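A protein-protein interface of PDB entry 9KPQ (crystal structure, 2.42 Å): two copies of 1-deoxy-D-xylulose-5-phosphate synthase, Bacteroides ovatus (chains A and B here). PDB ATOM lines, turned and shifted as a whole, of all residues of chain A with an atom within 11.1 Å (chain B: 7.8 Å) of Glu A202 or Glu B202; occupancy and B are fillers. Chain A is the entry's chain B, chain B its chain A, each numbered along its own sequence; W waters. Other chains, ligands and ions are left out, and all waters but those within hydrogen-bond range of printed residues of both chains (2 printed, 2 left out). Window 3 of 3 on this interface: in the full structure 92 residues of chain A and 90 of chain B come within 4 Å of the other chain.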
ATOM      1  N   ARG A 189      12.957  14.949 -26.095  1.00  0.00           N
ATOM      2  CA  ARG A 189      12.012  15.465 -25.125  1.00  0.00           C
ATOM      3  C   ARG A 189      12.532  16.768 -24.477  1.00  0.00           C
ATOM      4  O   ARG A 189      11.743  17.685 -24.245  1.00  0.00           O
ATOM      5  CB  ARG A 189      11.698  14.395 -24.073  1.00  0.00           C
ATOM      6  CG  ARG A 189      10.963  13.205 -24.665  1.00  0.00           C
ATOM      7  CD  ARG A 189      10.295  12.326 -23.614  1.00  0.00           C
ATOM      8  NE  ARG A 189      11.231  11.837 -22.609  1.00  0.00           N
ATOM      9  CZ  ARG A 189      11.915  10.705 -22.706  1.00  0.00           C
ATOM     10  NH1 ARG A 189      11.819   9.930 -23.777  1.00  0.00           N
ATOM     11  NH2 ARG A 189      12.716  10.341 -21.707  1.00  0.00           N
ATOM     12  N   ASN A 190      13.838  16.870 -24.221  1.00  0.00           N
ATOM     13  CA  ASN A 190      14.427  18.107 -23.695  1.00  0.00           C
ATOM     14  C   ASN A 190      14.368  19.264 -24.721  1.00  0.00           C
ATOM     15  O   ASN A 190      14.168  20.441 -24.362  1.00  0.00           O
ATOM     16  CB  ASN A 190      15.873  17.868 -23.246  1.00  0.00           C
ATOM     17  CG  ASN A 190      16.504  19.104 -22.573  1.00  0.00           C
ATOM     18  OD1 ASN A 190      17.528  19.614 -23.024  1.00  0.00           O
ATOM     19  ND2 ASN A 190      15.895  19.573 -21.487  1.00  0.00           N
ATOM     20  N   LEU A 191      14.566  18.933 -25.993  1.00  0.00           N
ATOM     21  CA  LEU A 191      14.404  19.910 -27.061  1.00  0.00           C
ATOM     22  C   LEU A 191      12.969  20.466 -27.081  1.00  0.00           C
ATOM     23  O   LEU A 191      12.775  21.660 -27.271  1.00  0.00           O
ATOM     24  CB  LEU A 191      14.746  19.295 -28.427  1.00  0.00           C
ATOM     25  CG  LEU A 191      16.184  18.831 -28.684  1.00  0.00           C
ATOM     26  CD1 LEU A 191      16.352  18.534 -30.157  1.00  0.00           C
ATOM     27  CD2 LEU A 191      17.203  19.873 -28.221  1.00  0.00           C
ATOM     28  N   LYS A 192      11.971  19.597 -26.941  1.00  0.00           N
ATOM     29  CA  LYS A 192      10.585  20.057 -26.846  1.00  0.00           C
ATOM     30  C   LYS A 192      10.427  21.019 -25.664  1.00  0.00           C
ATOM     31  O   LYS A 192       9.792  22.064 -25.803  1.00  0.00           O
ATOM     32  CB  LYS A 192       9.602  18.893 -26.712  1.00  0.00           C
ATOM     33  CG  LYS A 192       8.167  19.301 -27.019  1.00  0.00           C
ATOM     34  CD  LYS A 192       7.154  18.354 -26.398  1.00  0.00           C
ATOM     35  CE  LYS A 192       5.765  18.976 -26.350  1.00  0.00           C
ATOM     36  NZ  LYS A 192       5.459  19.757 -27.586  1.00  0.00           N
ATOM     37  N   GLU A 193      11.030  20.674 -24.527  1.00  0.00           N
ATOM     38  CA  GLU A 193      10.994  21.512 -23.339  1.00  0.00           C
ATOM     39  C   GLU A 193      11.571  22.879 -23.697  1.00  0.00           C
ATOM     40  O   GLU A 193      10.986  23.906 -23.381  1.00  0.00           O
ATOM     41  CB  GLU A 193      11.798  20.904 -22.183  1.00  0.00           C
ATOM     42  CG  GLU A 193      11.189  19.700 -21.476  1.00  0.00           C
ATOM     43  CD  GLU A 193      12.138  19.099 -20.420  1.00  0.00           C
ATOM     44  OE1 GLU A 193      13.265  18.681 -20.774  1.00  0.00           O
ATOM     45  OE2 GLU A 193      11.763  19.047 -19.226  1.00  0.00           O
ATOM     46  N   LEU A 194      12.728  22.890 -24.359  1.00  0.00           N
ATOM     47  CA  LEU A 194      13.427  24.148 -24.642  1.00  0.00           C
ATOM     48  C   LEU A 194      12.594  25.039 -25.564  1.00  0.00           C
ATOM     49  O   LEU A 194      12.455  26.249 -25.328  1.00  0.00           O
ATOM     50  CB  LEU A 194      14.798  23.878 -25.267  1.00  0.00           C
ATOM     51  CG  LEU A 194      15.882  23.306 -24.351  1.00  0.00           C
ATOM     52  CD1 LEU A 194      17.055  22.756 -25.176  1.00  0.00           C
ATOM     53  CD2 LEU A 194      16.357  24.368 -23.377  1.00  0.00           C
ATOM     54  N   ARG A 195      12.031  24.435 -26.608  1.00  0.00           N
ATOM     55  CA  ARG A 195      11.203  25.168 -27.552  1.00  0.00           C
ATOM     56  C   ARG A 195       9.936  25.671 -26.867  1.00  0.00           C
ATOM     57  O   ARG A 195       9.526  26.803 -27.085  1.00  0.00           O
ATOM     58  CB  ARG A 195      10.855  24.300 -28.756  1.00  0.00           C
ATOM     59  CG  ARG A 195      12.070  23.902 -29.606  1.00  0.00           C
ATOM     60  CD  ARG A 195      11.652  23.236 -30.916  1.00  0.00           C
ATOM     61  NE  ARG A 195      10.569  22.268 -30.749  1.00  0.00           N
ATOM     62  CZ  ARG A 195      10.731  20.991 -30.423  1.00  0.00           C
ATOM     63  NH1 ARG A 195      11.933  20.461 -30.271  1.00  0.00           N
ATOM     64  NH2 ARG A 195       9.654  20.227 -30.248  1.00  0.00           N
ATOM     65  N   ASP A 196       9.308  24.822 -26.055  1.00  0.00           N
ATOM     66  CA  ASP A 196       8.054  25.174 -25.377  1.00  0.00           C
ATOM     67  C   ASP A 196       8.254  26.271 -24.328  1.00  0.00           C
ATOM     68  O   ASP A 196       7.333  27.023 -24.020  1.00  0.00           O
ATOM     69  CB  ASP A 196       7.437  23.936 -24.704  1.00  0.00           C
ATOM     70  CG  ASP A 196       6.720  23.022 -25.689  1.00  0.00           C
ATOM     71  OD1 ASP A 196       6.613  23.396 -26.879  1.00  0.00           O
ATOM     72  OD2 ASP A 196       6.264  21.932 -25.264  1.00  0.00           O
ATOM     73  N   SER A 197       9.461  26.359 -23.780  1.00  0.00           N
ATOM     74  CA  SER A 197       9.785  27.386 -22.797  1.00  0.00           C
ATOM     75  C   SER A 197      10.560  28.550 -23.422  1.00  0.00           C
ATOM     76  O   SER A 197      11.189  29.330 -22.707  1.00  0.00           O
ATOM     77  CB  SER A 197      10.590  26.779 -21.655  1.00  0.00           C
ATOM     78  OG  SER A 197      11.924  26.548 -22.065  1.00  0.00           O
ATOM     79  N   ASN A 198      10.547  28.633 -24.753  1.00  0.00           N
ATOM     80  CA  ASN A 198      11.329  29.628 -25.504  1.00  0.00           C
ATOM     81  C   ASN A 198      12.792  29.750 -24.995  1.00  0.00           C
ATOM     82  O   ASN A 198      13.320  30.848 -24.815  1.00  0.00           O
ATOM     83  CB  ASN A 198      10.620  30.986 -25.474  1.00  0.00           C
ATOM     84  CG  ASN A 198      11.196  31.965 -26.481  1.00  0.00           C
ATOM     85  OD1 ASN A 198      10.990  31.829 -27.685  1.00  0.00           O
ATOM     86  ND2 ASN A 198      11.917  32.968 -25.990  1.00  0.00           N
ATOM     87  N   GLY A 199      13.437  28.599 -24.800  1.00  0.00           N
ATOM     88  CA  GLY A 199      14.839  28.520 -24.425  1.00  0.00           C
ATOM     89  C   GLY A 199      15.189  28.831 -22.981  1.00  0.00           C
ATOM     90  O   GLY A 199      16.366  28.918 -22.623  1.00  0.00           O
ATOM     91  N   GLN A 200      14.179  28.961 -22.128  1.00  0.00           N
ATOM     92  CA  GLN A 200      14.434  29.409 -20.768  1.00  0.00           C
ATOM     93  C   GLN A 200      14.537  28.236 -19.779  1.00  0.00           C
ATOM     94  O   GLN A 200      15.079  28.405 -18.689  1.00  0.00           O
ATOM     95  CB  GLN A 200      13.363  30.406 -20.332  1.00  0.00           C
ATOM     96  CG  GLN A 200      13.011  31.392 -21.437  1.00  0.00           C
ATOM     97  CD  GLN A 200      11.740  32.198 -21.174  1.00  0.00           C
ATOM     98  OE1 GLN A 200      10.794  31.733 -20.528  1.00  0.00           O
ATOM     99  NE2 GLN A 200      11.694  33.394 -21.731  1.00  0.00           N
ATOM    100  N   CYS A 201      14.085  27.052 -20.172  1.00  0.00           N
ATOM    101  CA  CYS A 201      14.053  25.889 -19.292  1.00  0.00           C
ATOM    102  C   CYS A 201      15.394  25.633 -18.599  1.00  0.00           C
ATOM    103  O   CYS A 201      16.426  25.714 -19.262  1.00  0.00           O
ATOM    104  CB  CYS A 201      13.680  24.645 -20.131  1.00  0.00           C
ATOM    105  SG  CYS A 201      13.064  23.230 -19.238  1.00  0.00           S
ATOM    106  N   GLU A 202      15.398  25.266 -17.298  1.00  0.00           N
ATOM    107  CA  GLU A 202      16.661  25.115 -16.504  1.00  0.00           C
ATOM    108  C   GLU A 202      17.399  23.903 -17.044  1.00  0.00           C
ATOM    109  O   GLU A 202      18.626  23.878 -17.138  1.00  0.00           O
ATOM    110  CB  GLU A 202      16.548  24.819 -14.998  1.00  0.00           C
ATOM    111  CG  GLU A 202      15.959  25.766 -14.045  1.00  0.00           C
ATOM    112  CD  GLU A 202      14.771  25.237 -13.364  1.00  0.00           C
ATOM    113  OE1 GLU A 202      14.776  24.061 -12.996  1.00  0.00           O
ATOM    114  OE2 GLU A 202      13.724  25.960 -13.274  1.00  0.00           O
ATOM    115  N   CYS A 203      16.627  22.862 -17.362  1.00  0.00           N
ATOM    116  CA  CYS A 203      17.262  21.624 -17.777  1.00  0.00           C
ATOM    117  C   CYS A 203      17.658  21.693 -19.244  1.00  0.00           C
ATOM    118  O   CYS A 203      16.845  21.428 -20.143  1.00  0.00           O
ATOM    119  CB  CYS A 203      16.368  20.420 -17.539  1.00  0.00           C
ATOM    120  SG  CYS A 203      17.307  18.870 -17.431  1.00  0.00           S
ATOM    121  N   ASN A 204      18.923  22.052 -19.472  1.00  0.00           N
ATOM    122  CA  ASN A 204      19.420  22.283 -20.820  1.00  0.00           C
ATOM    123  C   ASN A 204      20.592  21.343 -21.171  1.00  0.00           C
ATOM    124  O   ASN A 204      21.701  21.499 -20.652  1.00  0.00           O
ATOM    125  CB  ASN A 204      19.830  23.753 -20.944  1.00  0.00           C
ATOM    126  CG  ASN A 204      20.025  24.212 -22.383  1.00  0.00           C
ATOM    127  OD1 ASN A 204      20.739  23.579 -23.172  1.00  0.00           O
ATOM    128  ND2 ASN A 204      19.431  25.357 -22.716  1.00  0.00           N
ATOM    129  N   PHE A 205      20.344  20.410 -22.091  1.00  0.00           N
ATOM    130  CA  PHE A 205      21.356  19.465 -22.588  1.00  0.00           C
ATOM    131  C   PHE A 205      22.633  20.169 -23.035  1.00  0.00           C
ATOM    132  O   PHE A 205      23.739  19.745 -22.692  1.00  0.00           O
ATOM    133  CB  PHE A 205      20.791  18.635 -23.749  1.00  0.00           C
ATOM    134  CG  PHE A 205      21.846  17.947 -24.583  1.00  0.00           C
ATOM    135  CD1 PHE A 205      22.512  16.825 -24.100  1.00  0.00           C
ATOM    136  CD2 PHE A 205      22.157  18.405 -25.868  1.00  0.00           C
ATOM    137  CE1 PHE A 205      23.485  16.183 -24.878  1.00  0.00           C
ATOM    138  CE2 PHE A 205      23.129  17.765 -26.648  1.00  0.00           C
ATOM    139  CZ  PHE A 205      23.787  16.650 -26.145  1.00  0.00           C
ATOM    140  N   PHE A 206      22.465  21.254 -23.786  1.00  0.00           N
ATOM    141  CA  PHE A 206      23.588  22.020 -24.295  1.00  0.00           C
ATOM    142  C   PHE A 206      24.427  22.654 -23.180  1.00  0.00           C
ATOM    143  O   PHE A 206      25.670  22.565 -23.198  1.00  0.00           O
ATOM    144  CB  PHE A 206      23.064  23.086 -25.268  1.00  0.00           C
ATOM    145  CG  PHE A 206      22.370  22.498 -26.494  1.00  0.00           C
ATOM    146  CD1 PHE A 206      23.093  21.750 -27.434  1.00  0.00           C
ATOM    147  CD2 PHE A 206      21.009  22.651 -26.685  1.00  0.00           C
ATOM    148  CE1 PHE A 206      22.457  21.192 -28.553  1.00  0.00           C
ATOM    149  CE2 PHE A 206      20.372  22.097 -27.795  1.00  0.00           C
ATOM    150  CZ  PHE A 206      21.103  21.372 -28.734  1.00  0.00           C
ATOM    151  N   LYS A 207      23.760  23.249 -22.182  1.00  0.00           N
ATOM    152  CA  LYS A 207      24.467  23.824 -21.027  1.00  0.00           C
ATOM    153  C   LYS A 207      25.079  22.711 -20.157  1.00  0.00           C
ATOM    154  O   LYS A 207      26.160  22.883 -19.594  1.00  0.00           O
ATOM    155  CB  LYS A 207      23.541  24.725 -20.200  1.00  0.00           C
ATOM    156  CG  LYS A 207      22.741  25.760 -21.040  1.00  0.00           C
ATOM    157  CD  LYS A 207      22.729  27.163 -20.431  1.00  0.00           C
ATOM    158  CE  LYS A 207      24.161  27.724 -20.329  1.00  0.00           C
ATOM    159  NZ  LYS A 207      24.200  29.220 -20.164  1.00  0.00           N
ATOM    160  N   ALA A 208      24.407  21.564 -20.058  1.00  0.00           N
ATOM    161  CA  ALA A 208      24.970  20.431 -19.322  1.00  0.00           C
ATOM    162  C   ALA A 208      26.285  19.957 -19.947  1.00  0.00           C
ATOM    163  O   ALA A 208      27.161  19.429 -19.250  1.00  0.00           O
ATOM    164  CB  ALA A 208      23.976  19.284 -19.257  1.00  0.00           C
ATOM    165  N   MET A 209      26.410  20.164 -21.260  1.00  0.00           N
ATOM    166  CA  MET A 209      27.615  19.799 -22.025  1.00  0.00           C
ATOM    167  C   MET A 209      28.759  20.811 -21.924  1.00  0.00           C
ATOM    168  O   MET A 209      29.836  20.581 -22.473  1.00  0.00           O
ATOM    169  CB  MET A 209      27.263  19.629 -23.512  1.00  0.00           C
ATOM    170  CG  MET A 209      26.453  18.391 -23.850  1.00  0.00           C
ATOM    171  SD  MET A 209      27.358  16.904 -23.414  1.00  0.00           S
ATOM    172  CE  MET A 209      28.501  16.827 -24.811  1.00  0.00           C
ATOM    173  N   GLY A 210      28.525  21.921 -21.229  1.00  0.00           N
ATOM    174  CA  GLY A 210      29.554  22.920 -21.012  1.00  0.00           C
ATOM    175  C   GLY A 210      29.422  24.137 -21.917  1.00  0.00           C
ATOM    176  O   GLY A 210      30.320  24.975 -21.987  1.00  0.00           O
ATOM    177  N   LEU A 211      28.279  24.269 -22.578  1.00  0.00           N
ATOM    178  CA  LEU A 211      28.141  25.278 -23.610  1.00  0.00           C
ATOM    179  C   LEU A 211      27.161  26.388 -23.250  1.00  0.00           C
ATOM    180  O   LEU A 211      26.188  26.178 -22.504  1.00  0.00           O
ATOM    181  CB  LEU A 211      27.692  24.611 -24.910  1.00  0.00           C
ATOM    182  CG  LEU A 211      28.656  23.590 -25.525  1.00  0.00           C
ATOM    183  CD1 LEU A 211      27.911  22.612 -26.413  1.00  0.00           C
ATOM    184  CD2 LEU A 211      29.722  24.288 -26.323  1.00  0.00           C
ATOM    185  N   TYR A 213      24.281  29.293 -24.543  1.00  0.00           N
ATOM    186  CA  TYR A 213      23.120  28.959 -25.338  1.00  0.00           C
ATOM    187  C   TYR A 213      22.140  30.110 -25.474  1.00  0.00           C
ATOM    188  O   TYR A 213      21.881  30.816 -24.508  1.00  0.00           O
ATOM    189  CB  TYR A 213      22.440  27.737 -24.703  1.00  0.00           C
ATOM    190  CG  TYR A 213      21.049  27.393 -25.182  1.00  0.00           C
ATOM    191  CD1 TYR A 213      19.919  28.023 -24.646  1.00  0.00           C
ATOM    192  CD2 TYR A 213      20.854  26.383 -26.123  1.00  0.00           C
ATOM    193  CE1 TYR A 213      18.642  27.682 -25.074  1.00  0.00           C
ATOM    194  CE2 TYR A 213      19.570  26.031 -26.540  1.00  0.00           C
ATOM    195  CZ  TYR A 213      18.479  26.689 -26.015  1.00  0.00           C
ATOM    196  OH  TYR A 213      17.218  26.354 -26.440  1.00  0.00           O
ATOM    197  N   ASN B 190      29.810  19.243 -15.680  1.00  0.00           N
ATOM    198  CA  ASN B 190      28.465  18.901 -15.212  1.00  0.00           C
ATOM    199  C   ASN B 190      28.430  17.855 -14.134  1.00  0.00           C
ATOM    200  O   ASN B 190      27.724  18.007 -13.127  1.00  0.00           O
ATOM    201  CB  ASN B 190      27.522  18.457 -16.332  1.00  0.00           C
ATOM    202  CG  ASN B 190      26.030  18.348 -15.848  1.00  0.00           C
ATOM    203  OD1 ASN B 190      25.436  17.281 -15.943  1.00  0.00           O
ATOM    204  ND2 ASN B 190      25.430  19.458 -15.396  1.00  0.00           N
ATOM    205  N   GLU B 193      29.397  19.652 -11.009  1.00  0.00           N
ATOM    206  CA  GLU B 193      28.443  20.572 -10.317  1.00  0.00           C
ATOM    207  C   GLU B 193      27.464  19.714  -9.532  1.00  0.00           C
ATOM    208  O   GLU B 193      26.993  20.159  -8.468  1.00  0.00           O
ATOM    209  CB  GLU B 193      27.637  21.399 -11.317  1.00  0.00           C
ATOM    210  CG  GLU B 193      28.473  22.286 -12.216  1.00  0.00           C
ATOM    211  CD  GLU B 193      28.007  22.287 -13.662  1.00  0.00           C
ATOM    212  OE1 GLU B 193      26.924  21.730 -13.933  1.00  0.00           O
ATOM    213  OE2 GLU B 193      28.733  22.834 -14.515  1.00  0.00           O
ATOM    214  N   LEU B 194      27.172  18.516 -10.099  1.00  0.00           N
ATOM    215  CA  LEU B 194      26.264  17.575  -9.492  1.00  0.00           C
ATOM    216  C   LEU B 194      26.772  16.942  -8.221  1.00  0.00           C
ATOM    217  O   LEU B 194      25.984  16.711  -7.301  1.00  0.00           O
ATOM    218  CB  LEU B 194      25.927  16.473 -10.503  1.00  0.00           C
ATOM    219  CG  LEU B 194      24.933  16.737 -11.651  1.00  0.00           C
ATOM    220  CD1 LEU B 194      24.981  15.573 -12.645  1.00  0.00           C
ATOM    221  CD2 LEU B 194      23.498  16.965 -11.157  1.00  0.00           C
ATOM    222  N   SER B 197      26.442  19.547  -5.634  1.00  0.00           N
ATOM    223  CA  SER B 197      25.078  19.890  -5.247  1.00  0.00           C
ATOM    224  C   SER B 197      24.389  18.658  -4.662  1.00  0.00           C
ATOM    225  O   SER B 197      23.162  18.634  -4.467  1.00  0.00           O
ATOM    226  CB  SER B 197      24.296  20.431  -6.442  1.00  0.00           C
ATOM    227  OG  SER B 197      24.003  19.405  -7.370  1.00  0.00           O
ATOM    228  N   GLY B 199      23.699  15.902  -6.069  1.00  0.00           N
ATOM    229  CA  GLY B 199      22.714  15.355  -6.981  1.00  0.00           C
ATOM    230  C   GLY B 199      21.456  16.187  -7.122  1.00  0.00           C
ATOM    231  O   GLY B 199      20.456  15.730  -7.681  1.00  0.00           O
ATOM    232  N   GLN B 200      21.497  17.406  -6.600  1.00  0.00           N
ATOM    233  CA  GLN B 200      20.297  18.221  -6.521  1.00  0.00           C
ATOM    234  C   GLN B 200      20.209  19.180  -7.696  1.00  0.00           C
ATOM    235  O   GLN B 200      19.124  19.673  -8.013  1.00  0.00           O
ATOM    236  CB  GLN B 200      20.278  19.000  -5.206  1.00  0.00           C
ATOM    237  CG  GLN B 200      19.352  18.439  -4.139  1.00  0.00           C
ATOM    238  CD  GLN B 200      19.672  18.986  -2.744  1.00  0.00           C
ATOM    239  OE1 GLN B 200      20.035  20.156  -2.584  1.00  0.00           O
ATOM    240  NE2 GLN B 200      19.536  18.134  -1.727  1.00  0.00           N
ATOM    241  N   CYS B 201      21.332  19.408  -8.373  1.00  0.00           N
ATOM    242  CA  CYS B 201      21.374  20.434  -9.418  1.00  0.00           C
ATOM    243  C   CYS B 201      20.335  20.262 -10.519  1.00  0.00           C
ATOM    244  O   CYS B 201      20.013  19.152 -10.970  1.00  0.00           O
ATOM    245  CB  CYS B 201      22.743  20.507 -10.078  1.00  0.00           C
ATOM    246  SG  CYS B 201      22.819  21.844 -11.317  1.00  0.00           S
ATOM    247  N   GLU B 202      19.714  21.390 -10.851  1.00  0.00           N
ATOM    248  CA  GLU B 202      18.662  21.441 -11.853  1.00  0.00           C
ATOM    249  C   GLU B 202      19.202  21.035 -13.206  1.00  0.00           C
ATOM    250  O   GLU B 202      18.651  20.156 -13.867  1.00  0.00           O
ATOM    251  CB  GLU B 202      18.058  22.844 -11.926  1.00  0.00           C
ATOM    252  CG  GLU B 202      16.834  23.040 -11.048  1.00  0.00           C
ATOM    253  CD  GLU B 202      16.817  24.395 -10.367  1.00  0.00           C
ATOM    254  OE1 GLU B 202      16.597  25.407 -11.064  1.00  0.00           O
ATOM    255  OE2 GLU B 202      17.021  24.446  -9.136  1.00  0.00           O
ATOM    256  N   CYS B 203      20.284  21.681 -13.620  1.00  0.00           N
ATOM    257  CA  CYS B 203      20.880  21.345 -14.923  1.00  0.00           C
ATOM    258  C   CYS B 203      21.674  20.025 -14.823  1.00  0.00           C
ATOM    259  O   CYS B 203      22.868  19.998 -14.466  1.00  0.00           O
ATOM    260  CB  CYS B 203      21.793  22.456 -15.425  1.00  0.00           C
ATOM    261  SG  CYS B 203      22.016  22.468 -17.229  1.00  0.00           S
ATOM    262  N   ASN B 204      20.990  18.937 -15.149  1.00  0.00           N
ATOM    263  CA  ASN B 204      21.508  17.597 -14.993  1.00  0.00           C
ATOM    264  C   ASN B 204      21.583  16.965 -16.375  1.00  0.00           C
ATOM    265  O   ASN B 204      20.549  16.791 -17.033  1.00  0.00           O
ATOM    266  CB  ASN B 204      20.597  16.808 -14.051  1.00  0.00           C
ATOM    267  CG  ASN B 204      21.089  15.388 -13.765  1.00  0.00           C
ATOM    268  OD1 ASN B 204      21.547  14.655 -14.659  1.00  0.00           O
ATOM    269  ND2 ASN B 204      20.936  14.977 -12.511  1.00  0.00           N
ATOM    270  N   PHE B 205      22.802  16.667 -16.828  1.00  0.00           N
ATOM    271  CA  PHE B 205      23.001  16.016 -18.118  1.00  0.00           C
ATOM    272  C   PHE B 205      22.123  14.770 -18.297  1.00  0.00           C
ATOM    273  O   PHE B 205      21.456  14.610 -19.325  1.00  0.00           O
ATOM    274  CB  PHE B 205      24.462  15.627 -18.283  1.00  0.00           C
ATOM    275  CG  PHE B 205      24.721  14.695 -19.443  1.00  0.00           C
ATOM    276  CD1 PHE B 205      24.661  15.161 -20.747  1.00  0.00           C
ATOM    277  CD2 PHE B 205      25.047  13.359 -19.223  1.00  0.00           C
ATOM    278  CE1 PHE B 205      24.917  14.313 -21.812  1.00  0.00           C
ATOM    279  CE2 PHE B 205      25.304  12.506 -20.284  1.00  0.00           C
ATOM    280  CZ  PHE B 205      25.239  12.987 -21.581  1.00  0.00           C
ATOM    281  N   LYS B 207      19.303  13.868 -16.766  1.00  0.00           N
ATOM    282  CA  LYS B 207      17.887  14.224 -16.882  1.00  0.00           C
ATOM    283  C   LYS B 207      17.602  14.892 -18.243  1.00  0.00           C
ATOM    284  O   LYS B 207      16.538  14.686 -18.832  1.00  0.00           O
ATOM    285  CB  LYS B 207      17.460  15.169 -15.741  1.00  0.00           C
ATOM    286  CG  LYS B 207      17.309  14.541 -14.343  1.00  0.00           C
ATOM    287  CD  LYS B 207      15.954  13.839 -14.129  1.00  0.00           C
ATOM    288  CE  LYS B 207      14.850  14.381 -15.041  1.00  0.00           C
ATOM    289  NZ  LYS B 207      13.518  13.701 -14.872  1.00  0.00           N
ATOM    290  N   ALA B 208      18.551  15.692 -18.735  1.00  0.00           N
ATOM    291  CA  ALA B 208      18.450  16.326 -20.057  1.00  0.00           C
ATOM    292  C   ALA B 208      18.375  15.274 -21.157  1.00  0.00           C
ATOM    293  O   ALA B 208      17.726  15.481 -22.195  1.00  0.00           O
ATOM    294  CB  ALA B 208      19.641  17.256 -20.300  1.00  0.00           C
HETATM  295  O   HOH W   1      13.614  15.818 -20.152  1.00  0.00           O
HETATM  296  O   HOH W   2      24.590  22.571 -16.612  1.00  0.00           O
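Of the 24 printed residues of chain A, 7 touch a printed residue of chain B. Printed residues of chain A that touch a printed residue of chain B: Asn A190, Glu A202, Cys A203, Asn A204, Phe A205, Ala A208 and Met A209. Of the 13 printed residues of chain B, 6 touch a printed residue of chain A. Hydrophobic or aromatic side chains of chain B that line the printed part of chain A: Phe B205 and Ala B208. Among the printed residues, no Asp or Glu carboxylate lies within 4 Å of a Lys or Arg side-chain nitrogen of the other chain.
O of Glu A202 is in hydrogen-bond range of SG of Cys B203, at 3.7 Å. The side-chain carboxylate (OE1) of Glu A202 sits close to the side-chain carboxylate (OE1) of Glu B202. The side-chain sulfur of Cys B203 lies within hydrogen-bond range of the backbone carbonyl oxygen of Asn A204 (3.6 Å). N of Ala B208 is in hydrogen-bond range of SG of Cys A203 (3.7 Å).
Asn A190 touches Ala B208, and with the chains exchanged Ala A208 touches Asn B190. Glu A202 touches Cys B203, but with the chains exchanged Cys A203 does not touch Glu B202 (4.02 Å). Cys A203 touches Asn B204, and with the chains exchanged Asn A204 touches Cys B203. Phe A205 touches Ala B208, and with the chains exchanged Ala A208 touches Phe B205. Positions printed for both chains: 190, 193, 194, 197, 199, 200, 201, 202, 203, 204, 205, 207 and 208.
Water W2 lies within hydrogen-bond range of the side-chain sulfur (SG) of Cys B203, the backbone carbonyl oxygen (O) of Lys A207 and the side-chain amide nitrogen (ND2) of Asn B190. Water W1 lies within hydrogen-bond range of OE1 of Glu A193 (3.0 Å) and O of Lys B207 (3.4 Å).
Of the printed residues of chain B, Asn A190 touches Ala B208. No residue of chain B comes within 4 Å of Cys A201. Glu A202 touches just these residues of chain B: Glu B202 and Cys B203. Of the printed residues of chain B, Ala A208 touches Asn B190 (3.1 Å), Cys B203 (3.8 Å) and Phe B205 (3.6 Å). Printed residues of chain B within 4 Å of Met A209: Phe B205. No residue of chain A comes within 4 Å of Cys B201. Of chain A, only Glu A202, Asn A204 and Ala A208 come within 4 Å of Cys B203. Of chain A, only Cys A203 comes within 4 Å of Asn B204. Printed residues of chain A within 4 Å of Phe B205: Phe A205 (3.9 Å), Ala A208 (3.6 Å) and Met A209 (3.9 Å). The nearest printed residue of chain B that does not touch Asn A204 is Ala B208 (4.3 Å).
The side-chain amide oxygen (OD1) of Asn A204 sits at hydrogen-bond distance from the backbone NH (N) of Lys A207, 3.2 Å away. The side-chain amide oxygen (OD1) of Asn A190 is in hydrogen-bond range of the backbone NH (N) of Phe A205 (3.1 Å). ND2 of Asn B190 sits at hydrogen-bond distance from O of Cys B203. The side-chain carboxylate of Glu A193 lies within hydrogen-bond range of the side-chain amide nitrogen of Asn A190 (2.9 Å). The side-chain amide oxygen of Asn B204 lies within hydrogen-bond range of the backbone NH of Lys B207. N of Phe A206 is in hydrogen-bond range of OD1 of Asn A204 (3.0 Å).
O of Ala B208 touches CB of Asn A190, 3.2 Å away. Asn B204 touches Cys A203. CE1 of Phe A205 touches CE1 of Phe B205, at 3.9 Å. Phe A205 touches Ala B208. Ala A208 touches Asn B190 (O to CB, 3.1 Å). Cys B203 touches Ala A208 (SG to N, 3.8 Å). CA of Phe B205 touches CB of Ala A208, at 3.6 Å. Met A209 touches Phe B205 (SD to CE1, 3.9 Å).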
